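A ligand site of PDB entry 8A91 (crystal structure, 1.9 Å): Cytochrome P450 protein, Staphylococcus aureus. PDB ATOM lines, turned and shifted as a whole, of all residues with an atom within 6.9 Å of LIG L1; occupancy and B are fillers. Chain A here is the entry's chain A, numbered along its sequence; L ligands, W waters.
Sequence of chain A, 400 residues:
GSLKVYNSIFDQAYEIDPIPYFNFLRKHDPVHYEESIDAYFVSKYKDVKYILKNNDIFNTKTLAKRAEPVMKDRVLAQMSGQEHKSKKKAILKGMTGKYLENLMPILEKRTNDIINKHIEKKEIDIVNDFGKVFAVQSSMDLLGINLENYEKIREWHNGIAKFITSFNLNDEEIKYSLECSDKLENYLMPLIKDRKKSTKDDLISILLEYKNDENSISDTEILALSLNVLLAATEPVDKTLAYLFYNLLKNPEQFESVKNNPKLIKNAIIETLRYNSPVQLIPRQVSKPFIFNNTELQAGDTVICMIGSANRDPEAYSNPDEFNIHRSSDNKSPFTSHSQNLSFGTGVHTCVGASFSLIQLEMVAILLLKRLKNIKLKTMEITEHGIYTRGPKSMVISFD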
ATOM      1  N   LEU A  63       3.324 -38.361 -25.508  1.00  0.00           N
ATOM      2  CA  LEU A  63       2.824 -37.591 -24.365  1.00  0.00           C
ATOM      3  C   LEU A  63       2.804 -38.433 -23.096  1.00  0.00           C
ATOM      4  O   LEU A  63       3.170 -37.956 -22.012  1.00  0.00           O
ATOM      5  CB  LEU A  63       1.432 -37.063 -24.685  1.00  0.00           C
ATOM      6  CG  LEU A  63       1.334 -36.075 -25.851  1.00  0.00           C
ATOM      7  CD1 LEU A  63      -0.046 -36.126 -26.491  1.00  0.00           C
ATOM      8  CD2 LEU A  63       1.656 -34.664 -25.371  1.00  0.00           C
ATOM      9  N   HIS A 157       0.651 -26.076  -9.910  1.00  0.00           N
ATOM     10  CA  HIS A 157       0.313 -26.221 -11.323  1.00  0.00           C
ATOM     11  C   HIS A 157       1.459 -25.762 -12.204  1.00  0.00           C
ATOM     12  O   HIS A 157       1.832 -26.437 -13.177  1.00  0.00           O
ATOM     13  CB  HIS A 157      -0.958 -25.437 -11.649  1.00  0.00           C
ATOM     14  CG  HIS A 157      -1.073 -25.050 -13.090  1.00  0.00           C
ATOM     15  ND1 HIS A 157      -0.510 -23.899 -13.591  1.00  0.00           N
ATOM     16  CD2 HIS A 157      -1.669 -25.663 -14.139  1.00  0.00           C
ATOM     17  CE1 HIS A 157      -0.763 -23.816 -14.885  1.00  0.00           C
ATOM     18  NE2 HIS A 157      -1.469 -24.878 -15.238  1.00  0.00           N
ATOM     19  N   ALA A 161       3.228 -27.871 -14.944  1.00  0.00           N
ATOM     20  CA  ALA A 161       3.190 -27.513 -16.360  1.00  0.00           C
ATOM     21  C   ALA A 161       4.587 -27.369 -16.934  1.00  0.00           C
ATOM     22  O   ALA A 161       4.845 -27.809 -18.057  1.00  0.00           O
ATOM     23  CB  ALA A 161       2.388 -26.230 -16.545  1.00  0.00           C
ATOM     24  N   ILE A 164       5.773 -30.578 -18.261  1.00  0.00           N
ATOM     25  CA  ILE A 164       5.110 -31.067 -19.475  1.00  0.00           C
ATOM     26  C   ILE A 164       5.545 -30.261 -20.693  1.00  0.00           C
ATOM     27  O   ILE A 164       5.672 -30.810 -21.797  1.00  0.00           O
ATOM     28  CB  ILE A 164       3.580 -31.046 -19.297  1.00  0.00           C
ATOM     29  CG1 ILE A 164       3.162 -31.909 -18.107  1.00  0.00           C
ATOM     30  CG2 ILE A 164       2.886 -31.496 -20.573  1.00  0.00           C
ATOM     31  CD1 ILE A 164       2.721 -33.300 -18.495  1.00  0.00           C
ATOM     32  N   THR A 165       5.779 -28.967 -20.518  1.00  0.00           N
ATOM     33  CA  THR A 165       5.994 -28.058 -21.644  1.00  0.00           C
ATOM     34  C   THR A 165       7.467 -27.729 -21.867  1.00  0.00           C
ATOM     35  O   THR A 165       7.769 -26.871 -22.706  1.00  0.00           O
ATOM     36  CB  THR A 165       5.206 -26.766 -21.431  1.00  0.00           C
ATOM     37  OG1 THR A 165       5.822 -25.989 -20.402  1.00  0.00           O
ATOM     38  CG2 THR A 165       3.774 -27.084 -21.041  1.00  0.00           C
ATOM     39  N   ASN A 228      -4.991 -33.671 -15.205  1.00  0.00           N
ATOM     40  CA  ASN A 228      -5.056 -33.427 -16.636  1.00  0.00           C
ATOM     41  C   ASN A 228      -5.917 -32.200 -16.951  1.00  0.00           C
ATOM     42  O   ASN A 228      -5.510 -31.325 -17.719  1.00  0.00           O
ATOM     43  CB  ASN A 228      -5.612 -34.660 -17.356  1.00  0.00           C
ATOM     44  CG  ASN A 228      -5.530 -34.559 -18.861  1.00  0.00           C
ATOM     45  OD1 ASN A 228      -4.992 -33.595 -19.401  1.00  0.00           O
ATOM     46  ND2 ASN A 228      -6.058 -35.560 -19.549  1.00  0.00           N
ATOM     47  N   LEU A 231      -4.303 -28.861 -15.602  1.00  0.00           N
ATOM     48  CA  LEU A 231      -3.261 -28.384 -16.512  1.00  0.00           C
ATOM     49  C   LEU A 231      -3.859 -27.899 -17.827  1.00  0.00           C
ATOM     50  O   LEU A 231      -3.496 -26.819 -18.324  1.00  0.00           O
ATOM     51  CB  LEU A 231      -2.251 -29.494 -16.758  1.00  0.00           C
ATOM     52  CG  LEU A 231      -0.948 -29.410 -15.963  1.00  0.00           C
ATOM     53  CD1 LEU A 231      -0.071 -28.295 -16.499  1.00  0.00           C
ATOM     54  CD2 LEU A 231      -1.256 -29.180 -14.491  1.00  0.00           C
ATOM     55  N   ALA A 232      -4.785 -28.669 -18.398  1.00  0.00           N
ATOM     56  CA  ALA A 232      -5.298 -28.352 -19.727  1.00  0.00           C
ATOM     57  C   ALA A 232      -6.049 -27.029 -19.743  1.00  0.00           C
ATOM     58  O   ALA A 232      -5.915 -26.239 -20.683  1.00  0.00           O
ATOM     59  CB  ALA A 232      -6.196 -29.488 -20.220  1.00  0.00           C
ATOM     60  N   ALA A 233      -6.843 -26.771 -18.705  1.00  0.00           N
ATOM     61  CA  ALA A 233      -7.726 -25.606 -18.704  1.00  0.00           C
ATOM     62  C   ALA A 233      -7.049 -24.332 -18.226  1.00  0.00           C
ATOM     63  O   ALA A 233      -7.421 -23.239 -18.672  1.00  0.00           O
ATOM     64  CB  ALA A 233      -8.951 -25.880 -17.827  1.00  0.00           C
ATOM     65  N   THR A 234      -6.069 -24.442 -17.332  1.00  0.00           N
ATOM     66  CA  THR A 234      -5.475 -23.239 -16.735  1.00  0.00           C
ATOM     67  C   THR A 234      -4.533 -22.538 -17.693  1.00  0.00           C
ATOM     68  O   THR A 234      -4.697 -21.338 -17.974  1.00  0.00           O
ATOM     69  CB  THR A 234      -4.734 -23.615 -15.446  1.00  0.00           C
ATOM     70  OG1 THR A 234      -5.623 -24.315 -14.563  1.00  0.00           O
ATOM     71  CG2 THR A 234      -4.224 -22.373 -14.744  1.00  0.00           C
ATOM     72  N   GLU A 235      -3.557 -23.259 -18.234  1.00  0.00           N
ATOM     73  CA  GLU A 235      -2.436 -22.617 -18.919  1.00  0.00           C
ATOM     74  C   GLU A 235      -2.868 -21.743 -20.092  1.00  0.00           C
ATOM     75  O   GLU A 235      -2.385 -20.599 -20.184  1.00  0.00           O
ATOM     76  CB  GLU A 235      -1.447 -23.701 -19.365  1.00  0.00           C
ATOM     77  CG  GLU A 235      -0.315 -23.189 -20.228  1.00  0.00           C
ATOM     78  CD  GLU A 235       0.995 -23.141 -19.460  1.00  0.00           C
ATOM     79  OE1 GLU A 235       1.111 -23.871 -18.447  1.00  0.00           O
ATOM     80  OE2 GLU A 235       1.905 -22.390 -19.872  1.00  0.00           O
ATOM     81  N   PRO A 236      -3.739 -22.189 -21.004  1.00  0.00           N
ATOM     82  CA  PRO A 236      -4.009 -21.377 -22.203  1.00  0.00           C
ATOM     83  C   PRO A 236      -4.875 -20.147 -21.942  1.00  0.00           C
ATOM     84  O   PRO A 236      -4.880 -19.235 -22.785  1.00  0.00           O
ATOM     85  CB  PRO A 236      -4.737 -22.356 -23.132  1.00  0.00           C
ATOM     86  CG  PRO A 236      -4.530 -23.725 -22.514  1.00  0.00           C
ATOM     87  CD  PRO A 236      -4.439 -23.476 -21.053  1.00  0.00           C
ATOM     88  N   VAL A 279      -1.127 -22.583 -27.412  1.00  0.00           N
ATOM     89  CA  VAL A 279      -0.513 -23.901 -27.451  1.00  0.00           C
ATOM     90  C   VAL A 279       0.201 -24.019 -28.790  1.00  0.00           C
ATOM     91  O   VAL A 279      -0.433 -24.133 -29.843  1.00  0.00           O
ATOM     92  CB  VAL A 279      -1.543 -25.024 -27.265  1.00  0.00           C
ATOM     93  CG1 VAL A 279      -0.863 -26.388 -27.320  1.00  0.00           C
ATOM     94  CG2 VAL A 279      -2.284 -24.840 -25.940  1.00  0.00           C
ATOM     95  N   LEU A 281       2.815 -26.232 -29.795  1.00  0.00           N
ATOM     96  CA  LEU A 281       3.361 -27.501 -30.263  1.00  0.00           C
ATOM     97  C   LEU A 281       2.461 -28.660 -29.839  1.00  0.00           C
ATOM     98  O   LEU A 281       1.938 -28.670 -28.726  1.00  0.00           O
ATOM     99  CB  LEU A 281       4.780 -27.722 -29.707  1.00  0.00           C
ATOM    100  CG  LEU A 281       5.807 -26.606 -29.947  1.00  0.00           C
ATOM    101  CD1 LEU A 281       7.108 -26.928 -29.236  1.00  0.00           C
ATOM    102  CD2 LEU A 281       6.057 -26.414 -31.440  1.00  0.00           C
ATOM    103  N   ILE A 282       2.302 -29.620 -30.739  1.00  0.00           N
ATOM    104  CA  ILE A 282       1.600 -30.873 -30.440  1.00  0.00           C
ATOM    105  C   ILE A 282       2.470 -32.036 -30.888  1.00  0.00           C
ATOM    106  O   ILE A 282       2.677 -32.231 -32.100  1.00  0.00           O
ATOM    107  CB  ILE A 282       0.228 -30.930 -31.120  1.00  0.00           C
ATOM    108  CG1 ILE A 282      -0.704 -29.850 -30.587  1.00  0.00           C
ATOM    109  CG2 ILE A 282      -0.403 -32.296 -30.921  1.00  0.00           C
ATOM    110  CD1 ILE A 282      -2.025 -29.756 -31.330  1.00  0.00           C
ATOM    111  N   SER A 343      -5.944 -24.168 -33.519  1.00  0.00           N
ATOM    112  CA  SER A 343      -5.602 -23.765 -32.161  1.00  0.00           C
ATOM    113  C   SER A 343      -6.089 -24.757 -31.117  1.00  0.00           C
ATOM    114  O   SER A 343      -5.467 -24.895 -30.059  1.00  0.00           O
ATOM    115  CB  SER A 343      -6.178 -22.376 -31.869  1.00  0.00           C
ATOM    116  OG  SER A 343      -5.752 -21.438 -32.841  1.00  0.00           O
ATOM    117  N   CYS A 351      -9.338 -30.555 -28.647  1.00  0.00           N
ATOM    118  CA  CYS A 351      -9.561 -30.082 -27.290  1.00  0.00           C
ATOM    119  C   CYS A 351     -11.017 -30.278 -26.859  1.00  0.00           C
ATOM    120  O   CYS A 351     -11.937 -29.788 -27.515  1.00  0.00           O
ATOM    121  CB  CYS A 351      -9.176 -28.612 -27.180  1.00  0.00           C
ATOM    122  SG  CYS A 351      -9.485 -27.917 -25.538  1.00  0.00           S
ATOM    123  N   VAL A 352     -11.207 -30.991 -25.743  1.00  0.00           N
ATOM    124  CA  VAL A 352     -12.546 -31.203 -25.222  1.00  0.00           C
ATOM    125  C   VAL A 352     -13.159 -29.890 -24.716  1.00  0.00           C
ATOM    126  O   VAL A 352     -14.379 -29.730 -24.707  1.00  0.00           O
ATOM    127  CB  VAL A 352     -12.529 -32.266 -24.117  1.00  0.00           C
ATOM    128  CG1 VAL A 352     -11.879 -31.709 -22.857  1.00  0.00           C
ATOM    129  CG2 VAL A 352     -13.942 -32.757 -23.815  1.00  0.00           C
ATOM    130  N   GLY A 353     -12.320 -28.951 -24.302  1.00  0.00           N
ATOM    131  CA  GLY A 353     -12.803 -27.707 -23.725  1.00  0.00           C
ATOM    132  C   GLY A 353     -12.896 -26.553 -24.701  1.00  0.00           C
ATOM    133  O   GLY A 353     -12.910 -25.389 -24.273  1.00  0.00           O
ATOM    134  N   TYR A 388       6.595 -23.938 -26.246  1.00  0.00           N
ATOM    135  CA  TYR A 388       5.573 -24.978 -26.241  1.00  0.00           C
ATOM    136  C   TYR A 388       4.192 -24.357 -25.985  1.00  0.00           C
ATOM    137  O   TYR A 388       3.274 -24.515 -26.799  1.00  0.00           O
ATOM    138  CB  TYR A 388       5.918 -26.027 -25.176  1.00  0.00           C
ATOM    139  CG  TYR A 388       5.237 -27.372 -25.364  1.00  0.00           C
ATOM    140  CD1 TYR A 388       3.859 -27.497 -25.291  1.00  0.00           C
ATOM    141  CD2 TYR A 388       5.987 -28.520 -25.595  1.00  0.00           C
ATOM    142  CE1 TYR A 388       3.243 -28.721 -25.455  1.00  0.00           C
ATOM    143  CE2 TYR A 388       5.383 -29.744 -25.767  1.00  0.00           C
ATOM    144  CZ  TYR A 388       4.017 -29.844 -25.701  1.00  0.00           C
ATOM    145  OH  TYR A 388       3.404 -31.076 -25.860  1.00  0.00           O
ATOM    146  N   THR A 389       4.053 -23.652 -24.873  1.00  0.00           N
ATOM    147  CA  THR A 389       2.943 -22.736 -24.652  1.00  0.00           C
ATOM    148  C   THR A 389       3.520 -21.326 -24.559  1.00  0.00           C
ATOM    149  O   THR A 389       4.575 -21.122 -23.949  1.00  0.00           O
ATOM    150  CB  THR A 389       2.151 -23.081 -23.383  1.00  0.00           C
ATOM    151  OG1 THR A 389       2.977 -22.878 -22.231  1.00  0.00           O
ATOM    152  CG2 THR A 389       1.696 -24.531 -23.433  1.00  0.00           C
HETATM  153  C1  LIG L   1      -4.675 -27.271 -23.683  1.00  0.00           C
HETATM  154  C2  LIG L   1       0.273 -28.017 -21.732  1.00  0.00           C
HETATM  155  C3  LIG L   1      -3.328 -27.910 -23.862  1.00  0.00           C
HETATM  156  C4  LIG L   1      -1.156 -28.576 -23.526  1.00  0.00           C
HETATM  157  C5  LIG L   1      -2.200 -27.801 -22.973  1.00  0.00           C
HETATM  158  C6  LIG L   1      -1.973 -27.138 -21.764  1.00  0.00           C
HETATM  159  C7  LIG L   1      -2.925 -28.718 -24.881  1.00  0.00           C
HETATM  160  C8  LIG L   1       0.088 -28.686 -22.914  1.00  0.00           C
HETATM  161  C9  LIG L   1      -0.741 -27.244 -21.158  1.00  0.00           C
HETATM  162  N1  LIG L   1      -5.729 -28.245 -23.365  1.00  0.00           N
HETATM  163  N2  LIG L   1      -1.634 -29.127 -24.691  1.00  0.00           N
HETATM  164  C1  LG2 L   2      -6.515 -30.980 -25.926  1.00  0.00           C
HETATM  165  C2  LG2 L   2      -5.829 -26.264 -26.884  1.00  0.00           C
HETATM  166  C3  LG2 L   2      -8.727 -25.116 -23.163  1.00  0.00           C
HETATM  167  C4  LG2 L   2      -8.926 -29.779 -21.886  1.00  0.00           C
HETATM  168  C5  LG2 L   2      -6.100 -29.812 -26.537  1.00  0.00           C
HETATM  169  C6  LG2 L   2      -5.325 -29.697 -27.755  1.00  0.00           C
HETATM  170  C7  LG2 L   2      -5.149 -28.400 -28.019  1.00  0.00           C
HETATM  171  C8  LG2 L   2      -5.796 -27.642 -26.973  1.00  0.00           C
HETATM  172  C9  LG2 L   2      -4.372 -27.808 -29.219  1.00  0.00           C
HETATM  173  C10 LG2 L   2      -4.804 -30.875 -28.610  1.00  0.00           C
HETATM  174  C11 LG2 L   2      -3.681 -31.623 -27.902  1.00  0.00           C
HETATM  175  C12 LG2 L   2      -3.277 -32.822 -28.716  1.00  0.00           C
HETATM  176  O1  LG2 L   2      -2.352 -33.563 -28.300  1.00  0.00           O
HETATM  177  O2  LG2 L   2      -3.884 -33.042 -29.805  1.00  0.00           O
HETATM  178  C13 LG2 L   2      -6.578 -25.536 -25.981  1.00  0.00           C
HETATM  179  C14 LG2 L   2      -6.726 -24.101 -25.952  1.00  0.00           C
HETATM  180  C15 LG2 L   2      -7.522 -23.786 -24.917  1.00  0.00           C
HETATM  181  C16 LG2 L   2      -7.906 -25.013 -24.260  1.00  0.00           C
HETATM  182  C17 LG2 L   2      -6.046 -23.158 -26.972  1.00  0.00           C
HETATM  183  C18 LG2 L   2      -8.003 -22.383 -24.466  1.00  0.00           C
HETATM  184  C19 LG2 L   2      -7.866 -21.312 -25.244  1.00  0.00           C
HETATM  185  C20 LG2 L   2      -9.068 -26.266 -22.503  1.00  0.00           C
HETATM  186  C21 LG2 L   2     -10.006 -26.375 -21.406  1.00  0.00           C
HETATM  187  C22 LG2 L   2     -10.071 -27.656 -21.035  1.00  0.00           C
HETATM  188  C23 LG2 L   2      -9.180 -28.419 -21.901  1.00  0.00           C
HETATM  189  C24 LG2 L   2     -10.784 -25.198 -20.777  1.00  0.00           C
HETATM  190  C25 LG2 L   2     -10.968 -28.179 -19.891  1.00  0.00           C
HETATM  191  C26 LG2 L   2     -10.967 -29.476 -19.550  1.00  0.00           C
HETATM  192  C27 LG2 L   2      -8.307 -30.514 -22.870  1.00  0.00           C
HETATM  193  C28 LG2 L   2      -8.183 -31.965 -22.911  1.00  0.00           C
HETATM  194  C29 LG2 L   2      -7.516 -32.288 -24.028  1.00  0.00           C
HETATM  195  C30 LG2 L   2      -7.197 -31.075 -24.733  1.00  0.00           C
HETATM  196  C31 LG2 L   2      -8.715 -32.957 -21.858  1.00  0.00           C
HETATM  197  C32 LG2 L   2      -7.163 -33.726 -24.480  1.00  0.00           C
HETATM  198  C33 LG2 L   2      -8.152 -34.129 -25.561  1.00  0.00           C
HETATM  199  C34 LG2 L   2      -8.019 -35.586 -25.926  1.00  0.00           C
HETATM  200  O3  LG2 L   2      -6.943 -36.177 -25.665  1.00  0.00           O
HETATM  201  O4  LG2 L   2      -8.996 -36.139 -26.483  1.00  0.00           O
HETATM  202  N1  LG2 L   2      -6.374 -28.530 -26.093  1.00  0.00           N
HETATM  203  N2  LG2 L   2      -7.309 -26.064 -24.932  1.00  0.00           N
HETATM  204  N3  LG2 L   2      -8.589 -27.535 -22.776  1.00  0.00           N
HETATM  205  N4  LG2 L   2      -7.686 -30.011 -24.000  1.00  0.00           N
HETATM  206 FE1  LG2 L   2      -7.552 -28.056 -24.452  1.00  0.00          FE
HETATM  207  O   HOH W   1       0.521 -30.423 -26.795  1.00  0.00           O
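The side-chain hydroxyl (OG1) of Thr 165 lies within hydrogen-bond range of the backbone carbonyl oxygen (O) of Ala 161 (3.1 Å).
The backbone carbonyl oxygen of Ala 232 lies close to a nitrogen (N1) of LIG L1 (3.4 Å). An iron atom (FE1) of LG2 L2 is bound by the side-chain sulfur of Cys 351 (2.2 Å).
CG2 of Thr 165 touches C2 of LIG L1, 3.7 Å away. Leu 231 touches LIG L1 (O to C6, 3.8 Å). Pro 236 touches LIG L1. Val 279 touches LIG L1. Hydrophobic or aromatic side chains that line LIG L1: Ala 232, Pro 236 and Val 279.
A nitrogen (N1) of LIG L1 is bound to an iron atom (FE1) of LG2 L2.
Water W1 lies within hydrogen-bond range of O of Leu 281 (3.0 Å), OH of Tyr 388 (3.1 Å) and N2 of LIG L1 (3.3 Å).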
